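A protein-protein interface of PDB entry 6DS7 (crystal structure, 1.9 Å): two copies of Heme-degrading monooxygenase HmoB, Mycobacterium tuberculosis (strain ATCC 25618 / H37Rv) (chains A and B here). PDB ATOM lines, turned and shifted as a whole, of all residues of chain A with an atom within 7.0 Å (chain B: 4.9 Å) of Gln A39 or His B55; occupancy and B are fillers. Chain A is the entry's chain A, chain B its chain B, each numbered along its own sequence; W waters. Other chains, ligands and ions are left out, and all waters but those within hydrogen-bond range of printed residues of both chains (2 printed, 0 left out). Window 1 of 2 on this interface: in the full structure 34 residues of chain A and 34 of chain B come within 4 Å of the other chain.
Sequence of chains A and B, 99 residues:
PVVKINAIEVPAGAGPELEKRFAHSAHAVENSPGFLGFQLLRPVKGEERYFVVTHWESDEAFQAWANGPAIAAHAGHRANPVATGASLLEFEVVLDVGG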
ATOM      1  N   PHE A  22       9.465  22.180 -30.431  1.00  0.00           N
ATOM      2  CA  PHE A  22       8.239  22.263 -29.644  1.00  0.00           C
ATOM      3  C   PHE A  22       7.587  23.631 -29.639  1.00  0.00           C
ATOM      4  O   PHE A  22       6.461  23.742 -29.131  1.00  0.00           O
ATOM      5  CB  PHE A  22       8.509  21.845 -28.200  1.00  0.00           C
ATOM      6  CG  PHE A  22       8.542  20.382 -28.049  1.00  0.00           C
ATOM      7  CD1 PHE A  22       9.650  19.679 -28.448  1.00  0.00           C
ATOM      8  CD2 PHE A  22       7.442  19.686 -27.569  1.00  0.00           C
ATOM      9  CE1 PHE A  22       9.704  18.331 -28.322  1.00  0.00           C
ATOM     10  CE2 PHE A  22       7.499  18.322 -27.443  1.00  0.00           C
ATOM     11  CZ  PHE A  22       8.619  17.653 -27.844  1.00  0.00           C
ATOM     12  N   PHE A  35      -7.926  16.275 -23.053  1.00  0.00           N
ATOM     13  CA  PHE A  35      -6.584  16.784 -22.821  1.00  0.00           C
ATOM     14  C   PHE A  35      -6.608  17.776 -21.670  1.00  0.00           C
ATOM     15  O   PHE A  35      -7.411  18.710 -21.679  1.00  0.00           O
ATOM     16  CB  PHE A  35      -6.070  17.467 -24.082  1.00  0.00           C
ATOM     17  CG  PHE A  35      -4.757  18.197 -23.890  1.00  0.00           C
ATOM     18  CD1 PHE A  35      -3.578  17.478 -23.679  1.00  0.00           C
ATOM     19  CD2 PHE A  35      -4.688  19.580 -23.974  1.00  0.00           C
ATOM     20  CE1 PHE A  35      -2.345  18.141 -23.502  1.00  0.00           C
ATOM     21  CE2 PHE A  35      -3.454  20.251 -23.772  1.00  0.00           C
ATOM     22  CZ  PHE A  35      -2.289  19.516 -23.566  1.00  0.00           C
ATOM     23  N   GLY A  37      -3.426  19.149 -20.380  1.00  0.00           N
ATOM     24  CA  GLY A  37      -2.251  20.014 -20.425  1.00  0.00           C
ATOM     25  C   GLY A  37      -0.939  19.283 -20.644  1.00  0.00           C
ATOM     26  O   GLY A  37      -0.832  18.073 -20.487  1.00  0.00           O
ATOM     27  N   PHE A  38       0.082  20.044 -21.050  1.00  0.00           N
ATOM     28  CA  PHE A  38       1.384  19.434 -21.132  1.00  0.00           C
ATOM     29  C   PHE A  38       2.464  20.476 -20.859  1.00  0.00           C
ATOM     30  O   PHE A  38       2.234  21.684 -20.910  1.00  0.00           O
ATOM     31  CB  PHE A  38       1.578  18.684 -22.457  1.00  0.00           C
ATOM     32  CG  PHE A  38       2.320  19.429 -23.530  1.00  0.00           C
ATOM     33  CD1 PHE A  38       3.691  19.373 -23.624  1.00  0.00           C
ATOM     34  CD2 PHE A  38       1.609  20.082 -24.540  1.00  0.00           C
ATOM     35  CE1 PHE A  38       4.357  20.028 -24.699  1.00  0.00           C
ATOM     36  CE2 PHE A  38       2.252  20.733 -25.584  1.00  0.00           C
ATOM     37  CZ  PHE A  38       3.631  20.709 -25.649  1.00  0.00           C
ATOM     38  N   GLN A  39       3.592  19.968 -20.409  1.00  0.00           N
ATOM     39  CA  GLN A  39       4.797  20.766 -20.185  1.00  0.00           C
ATOM     40  C   GLN A  39       6.005  20.096 -20.817  1.00  0.00           C
ATOM     41  O   GLN A  39       6.191  18.876 -20.701  1.00  0.00           O
ATOM     42  CB  GLN A  39       5.053  20.963 -18.695  1.00  0.00           C
ATOM     43  CG  GLN A  39       3.997  21.808 -17.980  1.00  0.00           C
ATOM     44  CD  GLN A  39       4.432  22.296 -16.563  1.00  0.00           C
ATOM     45  OE1 GLN A  39       4.965  21.539 -15.749  1.00  0.00           O
ATOM     46  NE2 GLN A  39       4.155  23.552 -16.275  1.00  0.00           N
ATOM     47  N   LEU A  40       6.828  20.895 -21.488  1.00  0.00           N
ATOM     48  CA  LEU A  40       8.128  20.424 -21.936  1.00  0.00           C
ATOM     49  C   LEU A  40       9.115  20.778 -20.831  1.00  0.00           C
ATOM     50  O   LEU A  40       9.185  21.940 -20.442  1.00  0.00           O
ATOM     51  CB  LEU A  40       8.504  21.103 -23.261  1.00  0.00           C
ATOM     52  CG  LEU A  40       9.926  20.794 -23.753  1.00  0.00           C
ATOM     53  CD1 LEU A  40      10.090  19.299 -24.044  1.00  0.00           C
ATOM     54  CD2 LEU A  40      10.288  21.647 -24.958  1.00  0.00           C
ATOM     55  N   LEU A  41       9.809  19.778 -20.275  1.00  0.00           N
ATOM     56  CA  LEU A  41      10.688  19.983 -19.129  1.00  0.00           C
ATOM     57  C   LEU A  41      12.120  19.748 -19.562  1.00  0.00           C
ATOM     58  O   LEU A  41      12.469  18.637 -20.010  1.00  0.00           O
ATOM     59  CB  LEU A  41      10.334  19.060 -17.948  1.00  0.00           C
ATOM     60  CG  LEU A  41       8.897  19.187 -17.389  1.00  0.00           C
ATOM     61  CD1 LEU A  41       8.723  18.243 -16.168  1.00  0.00           C
ATOM     62  CD2 LEU A  41       8.528  20.587 -16.989  1.00  0.00           C
ATOM     63  N   PHE A  51      11.683  15.665 -20.448  1.00  0.00           N
ATOM     64  CA  PHE A  51      10.384  15.055 -20.157  1.00  0.00           C
ATOM     65  C   PHE A  51       9.285  15.864 -20.816  1.00  0.00           C
ATOM     66  O   PHE A  51       9.092  17.036 -20.478  1.00  0.00           O
ATOM     67  CB  PHE A  51      10.109  15.022 -18.644  1.00  0.00           C
ATOM     68  CG  PHE A  51      10.766  13.870 -17.906  1.00  0.00           C
ATOM     69  CD1 PHE A  51      11.755  13.112 -18.495  1.00  0.00           C
ATOM     70  CD2 PHE A  51      10.382  13.562 -16.600  1.00  0.00           C
ATOM     71  CE1 PHE A  51      12.374  12.063 -17.808  1.00  0.00           C
ATOM     72  CE2 PHE A  51      10.973  12.543 -15.924  1.00  0.00           C
ATOM     73  CZ  PHE A  51      11.986  11.795 -16.494  1.00  0.00           C
ATOM     74  N   VAL A  52       8.517  15.230 -21.687  1.00  0.00           N
ATOM     75  CA  VAL A  52       7.293  15.798 -22.241  1.00  0.00           C
ATOM     76  C   VAL A  52       6.142  15.218 -21.420  1.00  0.00           C
ATOM     77  O   VAL A  52       5.773  14.041 -21.558  1.00  0.00           O
ATOM     78  CB  VAL A  52       7.147  15.482 -23.736  1.00  0.00           C
ATOM     79  CG1 VAL A  52       5.902  16.201 -24.302  1.00  0.00           C
ATOM     80  CG2 VAL A  52       8.424  15.909 -24.489  1.00  0.00           C
ATOM     81  N   VAL A  53       5.612  16.017 -20.502  1.00  0.00           N
ATOM     82  CA  VAL A  53       4.670  15.550 -19.501  1.00  0.00           C
ATOM     83  C   VAL A  53       3.272  15.958 -19.936  1.00  0.00           C
ATOM     84  O   VAL A  53       2.966  17.151 -19.992  1.00  0.00           O
ATOM     85  CB  VAL A  53       4.983  16.133 -18.124  1.00  0.00           C
ATOM     86  CG1 VAL A  53       4.087  15.461 -17.090  1.00  0.00           C
ATOM     87  CG2 VAL A  53       6.550  15.952 -17.797  1.00  0.00           C
ATOM     88  N   THR A  54       2.426  14.976 -20.253  1.00  0.00           N
ATOM     89  CA  THR A  54       1.061  15.259 -20.655  1.00  0.00           C
ATOM     90  C   THR A  54       0.084  14.653 -19.643  1.00  0.00           C
ATOM     91  O   THR A  54       0.303  13.570 -19.087  1.00  0.00           O
ATOM     92  CB  THR A  54       0.759  14.716 -22.064  1.00  0.00           C
ATOM     93  OG1 THR A  54       0.743  13.276 -22.047  1.00  0.00           O
ATOM     94  CG2 THR A  54       1.876  15.197 -23.037  1.00  0.00           C
ATOM     95  N   HIS A  55      -1.015  15.376 -19.459  1.00  0.00           N
ATOM     96  CA  HIS A  55      -2.044  15.054 -18.490  1.00  0.00           C
ATOM     97  C   HIS A  55      -3.339  14.816 -19.238  1.00  0.00           C
ATOM     98  O   HIS A  55      -3.691  15.598 -20.133  1.00  0.00           O
ATOM     99  CB  HIS A  55      -2.208  16.210 -17.531  1.00  0.00           C
ATOM    100  CG  HIS A  55      -0.970  16.555 -16.777  1.00  0.00           C
ATOM    101  ND1 HIS A  55      -0.877  16.391 -15.411  1.00  0.00           N
ATOM    102  CD2 HIS A  55       0.212  17.085 -17.181  1.00  0.00           C
ATOM    103  CE1 HIS A  55       0.306  16.811 -15.000  1.00  0.00           C
ATOM    104  NE2 HIS A  55       0.982  17.247 -16.048  1.00  0.00           N
ATOM    105  N   VAL A  97      -2.660  18.073  -5.713  1.00  0.00           N
ATOM    106  CA  VAL A  97      -2.726  19.108  -4.664  1.00  0.00           C
ATOM    107  C   VAL A  97      -2.393  20.446  -5.313  1.00  0.00           C
ATOM    108  O   VAL A  97      -1.331  20.587  -5.931  1.00  0.00           O
ATOM    109  CB  VAL A  97      -1.748  18.837  -3.497  1.00  0.00           C
ATOM    110  CG1 VAL A  97      -1.802  19.941  -2.466  1.00  0.00           C
ATOM    111  CG2 VAL A  97      -2.067  17.518  -2.827  1.00  0.00           C
ATOM    112  N   GLY A  99      -1.617  24.639  -5.605  1.00  0.00           N
ATOM    113  CA  GLY A  99      -0.659  25.539  -4.938  1.00  0.00           C
ATOM    114  C   GLY A  99      -1.230  26.120  -3.657  1.00  0.00           C
ATOM    115  O   GLY A  99      -0.871  25.594  -2.589  1.00  0.00           O
ATOM    116  N   VAL B   2       9.979  25.861 -12.094  1.00  0.00           N
ATOM    117  CA  VAL B   2      10.805  24.669 -12.093  1.00  0.00           C
ATOM    118  C   VAL B   2       9.909  23.516 -11.691  1.00  0.00           C
ATOM    119  O   VAL B   2       8.842  23.707 -11.090  1.00  0.00           O
ATOM    120  CB  VAL B   2      12.024  24.799 -11.139  1.00  0.00           C
ATOM    121  CG1 VAL B   2      12.971  25.896 -11.640  1.00  0.00           C
ATOM    122  CG2 VAL B   2      11.577  25.083  -9.737  1.00  0.00           C
ATOM    123  N   VAL B   3      10.346  22.319 -12.048  1.00  0.00           N
ATOM    124  CA  VAL B   3       9.704  21.074 -11.631  1.00  0.00           C
ATOM    125  C   VAL B   3      10.737  20.231 -10.924  1.00  0.00           C
ATOM    126  O   VAL B   3      11.858  20.074 -11.424  1.00  0.00           O
ATOM    127  CB  VAL B   3       9.120  20.292 -12.815  1.00  0.00           C
ATOM    128  CG1 VAL B   3       8.619  18.918 -12.323  1.00  0.00           C
ATOM    129  CG2 VAL B   3       7.961  21.102 -13.341  1.00  0.00           C
ATOM    130  N   GLY B  34       5.737  30.282  -3.166  1.00  0.00           N
ATOM    131  CA  GLY B  34       6.235  29.863  -4.469  1.00  0.00           C
ATOM    132  C   GLY B  34       5.833  28.451  -4.863  1.00  0.00           C
ATOM    133  O   GLY B  34       6.198  28.000  -5.973  1.00  0.00           O
ATOM    134  N   PHE B  35       5.126  27.729  -3.983  1.00  0.00           N
ATOM    135  CA  PHE B  35       4.652  26.399  -4.328  1.00  0.00           C
ATOM    136  C   PHE B  35       3.481  26.490  -5.295  1.00  0.00           C
ATOM    137  O   PHE B  35       2.480  27.169  -5.025  1.00  0.00           O
ATOM    138  CB  PHE B  35       4.218  25.655  -3.090  1.00  0.00           C
ATOM    139  CG  PHE B  35       3.682  24.289  -3.378  1.00  0.00           C
ATOM    140  CD1 PHE B  35       4.510  23.332  -3.898  1.00  0.00           C
ATOM    141  CD2 PHE B  35       2.348  23.967  -3.102  1.00  0.00           C
ATOM    142  CE1 PHE B  35       4.051  22.092  -4.188  1.00  0.00           C
ATOM    143  CE2 PHE B  35       1.873  22.689  -3.383  1.00  0.00           C
ATOM    144  CZ  PHE B  35       2.741  21.748  -3.889  1.00  0.00           C
ATOM    145  N   LEU B  36       3.573  25.761  -6.404  1.00  0.00           N
ATOM    146  CA  LEU B  36       2.500  25.761  -7.396  1.00  0.00           C
ATOM    147  C   LEU B  36       1.683  24.478  -7.423  1.00  0.00           C
ATOM    148  O   LEU B  36       0.779  24.371  -8.250  1.00  0.00           O
ATOM    149  CB  LEU B  36       3.064  26.014  -8.804  1.00  0.00           C
ATOM    150  CG  LEU B  36       3.911  27.284  -8.851  1.00  0.00           C
ATOM    151  CD1 LEU B  36       4.598  27.474 -10.247  1.00  0.00           C
ATOM    152  CD2 LEU B  36       3.009  28.506  -8.477  1.00  0.00           C
ATOM    153  N   GLY B  37       2.031  23.465  -6.632  1.00  0.00           N
ATOM    154  CA  GLY B  37       1.247  22.247  -6.679  1.00  0.00           C
ATOM    155  C   GLY B  37       2.048  20.963  -6.791  1.00  0.00           C
ATOM    156  O   GLY B  37       3.239  21.009  -7.162  1.00  0.00           O
ATOM    157  N   PHE B  38       1.420  19.812  -6.501  1.00  0.00           N
ATOM    158  CA  PHE B  38       2.117  18.552  -6.733  1.00  0.00           C
ATOM    159  C   PHE B  38       1.129  17.426  -6.982  1.00  0.00           C
ATOM    160  O   PHE B  38      -0.066  17.535  -6.681  1.00  0.00           O
ATOM    161  CB  PHE B  38       3.088  18.211  -5.595  1.00  0.00           C
ATOM    162  CG  PHE B  38       2.500  17.358  -4.439  1.00  0.00           C
ATOM    163  CD1 PHE B  38       1.904  17.956  -3.349  1.00  0.00           C
ATOM    164  CD2 PHE B  38       2.724  15.992  -4.402  1.00  0.00           C
ATOM    165  CE1 PHE B  38       1.448  17.190  -2.265  1.00  0.00           C
ATOM    166  CE2 PHE B  38       2.262  15.215  -3.359  1.00  0.00           C
ATOM    167  CZ  PHE B  38       1.617  15.826  -2.269  1.00  0.00           C
ATOM    168  N   VAL B  53       5.697  14.703  -8.313  1.00  0.00           N
ATOM    169  CA  VAL B  53       5.986  15.778  -9.245  1.00  0.00           C
ATOM    170  C   VAL B  53       5.611  17.099  -8.597  1.00  0.00           C
ATOM    171  O   VAL B  53       4.427  17.398  -8.401  1.00  0.00           O
ATOM    172  CB  VAL B  53       5.230  15.606 -10.571  1.00  0.00           C
ATOM    173  CG1 VAL B  53       5.620  16.808 -11.494  1.00  0.00           C
ATOM    174  CG2 VAL B  53       5.587  14.285 -11.173  1.00  0.00           C
ATOM    175  N   THR B  54       6.581  17.933  -8.278  1.00  0.00           N
ATOM    176  CA  THR B  54       6.223  19.195  -7.619  1.00  0.00           C
ATOM    177  C   THR B  54       6.612  20.372  -8.511  1.00  0.00           C
ATOM    178  O   THR B  54       7.588  20.309  -9.270  1.00  0.00           O
ATOM    179  CB  THR B  54       6.952  19.354  -6.234  1.00  0.00           C
ATOM    180  OG1 THR B  54       8.339  19.548  -6.504  1.00  0.00           O
ATOM    181  CG2 THR B  54       6.828  18.144  -5.406  1.00  0.00           C
ATOM    182  N   HIS B  55       5.856  21.457  -8.400  1.00  0.00           N
ATOM    183  CA  HIS B  55       5.999  22.646  -9.223  1.00  0.00           C
ATOM    184  C   HIS B  55       6.266  23.843  -8.342  1.00  0.00           C
ATOM    185  O   HIS B  55       5.605  24.014  -7.310  1.00  0.00           O
ATOM    186  CB  HIS B  55       4.726  22.921 -10.015  1.00  0.00           C
ATOM    187  CG  HIS B  55       4.344  21.776 -10.899  1.00  0.00           C
ATOM    188  ND1 HIS B  55       4.689  21.721 -12.231  1.00  0.00           N
ATOM    189  CD2 HIS B  55       3.689  20.620 -10.623  1.00  0.00           C
ATOM    190  CE1 HIS B  55       4.233  20.589 -12.751  1.00  0.00           C
ATOM    191  NE2 HIS B  55       3.617  19.907 -11.800  1.00  0.00           N
ATOM    192  N   TRP B  56       7.166  24.704  -8.807  1.00  0.00           N
ATOM    193  CA  TRP B  56       7.616  25.837  -8.018  1.00  0.00           C
ATOM    194  C   TRP B  56       7.896  27.009  -8.937  1.00  0.00           C
ATOM    195  O   TRP B  56       8.372  26.843 -10.078  1.00  0.00           O
ATOM    196  CB  TRP B  56       8.888  25.514  -7.189  1.00  0.00           C
ATOM    197  CG  TRP B  56       8.761  24.289  -6.288  1.00  0.00           C
ATOM    198  CD1 TRP B  56       9.004  22.987  -6.645  1.00  0.00           C
ATOM    199  CD2 TRP B  56       8.388  24.257  -4.889  1.00  0.00           C
ATOM    200  NE1 TRP B  56       8.801  22.158  -5.566  1.00  0.00           N
ATOM    201  CE2 TRP B  56       8.414  22.906  -4.484  1.00  0.00           C
ATOM    202  CE3 TRP B  56       8.075  25.240  -3.941  1.00  0.00           C
ATOM    203  CZ2 TRP B  56       8.097  22.512  -3.187  1.00  0.00           C
ATOM    204  CZ3 TRP B  56       7.720  24.848  -2.683  1.00  0.00           C
ATOM    205  CH2 TRP B  56       7.750  23.501  -2.301  1.00  0.00           C
ATOM    206  N   GLU B  57       7.675  28.202  -8.396  1.00  0.00           N
ATOM    207  CA  GLU B  57       8.054  29.403  -9.126  1.00  0.00           C
ATOM    208  C   GLU B  57       9.565  29.490  -9.318  1.00  0.00           C
ATOM    209  O   GLU B  57      10.027  30.039 -10.314  1.00  0.00           O
ATOM    210  CB  GLU B  57       7.536  30.633  -8.392  1.00  0.00           C
ATOM    211  CG  GLU B  57       7.663  31.880  -9.197  1.00  0.00           C
ATOM    212  CD  GLU B  57       6.989  31.737 -10.573  1.00  0.00           C
ATOM    213  OE1 GLU B  57       7.540  32.240 -11.589  1.00  0.00           O
ATOM    214  OE2 GLU B  57       5.917  31.096 -10.632  1.00  0.00           O
ATOM    215  N   VAL B  93      10.797  24.437 -16.524  1.00  0.00           N
ATOM    216  CA  VAL B  93       9.655  24.405 -17.431  1.00  0.00           C
ATOM    217  C   VAL B  93       9.991  25.261 -18.653  1.00  0.00           C
ATOM    218  O   VAL B  93      10.121  26.485 -18.550  1.00  0.00           O
ATOM    219  CB  VAL B  93       8.369  24.892 -16.761  1.00  0.00           C
ATOM    220  CG1 VAL B  93       7.256  24.910 -17.801  1.00  0.00           C
ATOM    221  CG2 VAL B  93       8.009  24.026 -15.574  1.00  0.00           C
ATOM    222  N   LEU B  95       8.097  24.948 -21.711  1.00  0.00           N
ATOM    223  CA  LEU B  95       6.879  25.250 -22.425  1.00  0.00           C
ATOM    224  C   LEU B  95       5.751  24.734 -21.573  1.00  0.00           C
ATOM    225  O   LEU B  95       5.860  23.645 -21.005  1.00  0.00           O
ATOM    226  CB  LEU B  95       6.882  24.567 -23.802  1.00  0.00           C
ATOM    227  CG  LEU B  95       5.689  24.832 -24.687  1.00  0.00           C
ATOM    228  CD1 LEU B  95       5.598  26.270 -25.099  1.00  0.00           C
ATOM    229  CD2 LEU B  95       5.857  23.913 -25.943  1.00  0.00           C
ATOM    230  N   ASP B  96       4.687  25.518 -21.450  1.00  0.00           N
ATOM    231  CA  ASP B  96       3.522  25.066 -20.694  1.00  0.00           C
ATOM    232  C   ASP B  96       2.287  25.336 -21.540  1.00  0.00           C
ATOM    233  O   ASP B  96       2.110  26.451 -22.043  1.00  0.00           O
ATOM    234  CB  ASP B  96       3.406  25.759 -19.334  1.00  0.00           C
ATOM    235  CG  ASP B  96       2.138  25.361 -18.592  1.00  0.00           C
ATOM    236  OD1 ASP B  96       2.156  24.335 -17.870  1.00  0.00           O
ATOM    237  OD2 ASP B  96       1.102  26.049 -18.769  1.00  0.00           O
HETATM  238  O   HOH W   1       2.928  17.747 -14.038  1.00  0.00           O
HETATM  239  O   HOH W   2      -0.022  22.647 -18.434  1.00  0.00           O
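Water W2 lies within hydrogen-bond range of OD1 of Asp B96 (2.8 Å) and O of Phe A38 (3.5 Å).
Water W1 bridges a ring nitrogen (NE2) of His A55 and a ring nitrogen (NE2) of His B55.
Hydrophobic or aromatic side chains of chain A that line the printed part of chain B: Phe A38, Leu A40, Leu A41 and Val A97.
Along chain B the printed residues that touch a printed residue of chain A span positions 3 to 96.
Among the printed residues, 17 pairs touch across the chains.
Among the printed residues, no Asp or Glu carboxylate lies within 4 Å of a Lys or Arg side-chain nitrogen of the other chain.
Of chain B, only Val B3 (3.9 Å), His B55 (3.2 Å), Val B93 (3.7 Å), Leu B95 (3.2 Å) and Asp B96 (2.7 Å) come within 4 Å of Gln A39.
Printed residues of chain A within 4 Å of His B55: Gln A39.
Printed residues of chain A within 4 Å of Leu B95: Phe A22 (3.2 Å), Phe A38 (3.9 Å), Gln A39 (3.2 Å) and Leu A40 (3.0 Å).
Of the printed residues of chain A, Leu B36 touches Gly A99 (3.6 Å).
Printed residues of chain A within 4 Å of Asp B96: Phe A38 (3.6 Å) and Gln A39 (2.7 Å).
Printed residues of chain A within 4 Å of Phe B38: Val A97.
Printed residues of chain B within 4 Å of Val A97: Gly B37 and Phe B38.
His A55 touches none of the printed residues of chain B.
The nearest printed residue of chain A that does not touch Gly B37 is Gln A39 (8.8 Å).
Among the printed residues, pairs that only touch across the chains: Val A97 with Gly B37 (3.2 Å), Gln A39 with Leu B95 (3.2 Å), Gln A39 with His B55 (3.2 Å), Phe A22 with Leu B95 (3.2 Å), Gly A99 with Phe B35 (3.5 Å), Gly A99 with Leu B36 (3.6 Å), Phe A38 with Asp B96 (3.6 Å), Gln A39 with Val B93 (3.7 Å), Leu A41 with Val B3 (3.7 Å), Leu A41 with Val B93 (3.8 Å), Gly A99 with Gly B37 (3.8 Å), Leu A40 with Val B93 (3.9 Å), Gln A39 with Val B3 (3.9 Å) and Phe A38 with Leu B95 (3.9 Å).
6 positions are printed for both chains.
Of the 17 pairs that touch across the chains among the printed residues, none has its exchanged pair printed and touching as well.
The backbone carbonyl oxygen of His B55 sits at hydrogen-bond distance from the backbone NH of Leu B36, at 2.8 Å.
N of Leu A41 sits at hydrogen-bond distance from O of Phe A51.
The backbone NH of His B55 sits at hydrogen-bond distance from the backbone carbonyl oxygen of Gly B37 (2.9 Å).
N of Gln A39 sits at hydrogen-bond distance from O of Val A53 (2.9 Å).
The backbone NH (N) of Val A97 lies within hydrogen-bond range of the backbone carbonyl oxygen (O) of Phe B38 (2.8 Å).
The backbone NH (N) of Leu A40 sits at hydrogen-bond distance from the backbone carbonyl oxygen (O) of Leu B95 (3.0 Å).
NE2 of Gln A39 is in hydrogen-bond range of OD1 of Asp B96 (2.7 Å).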
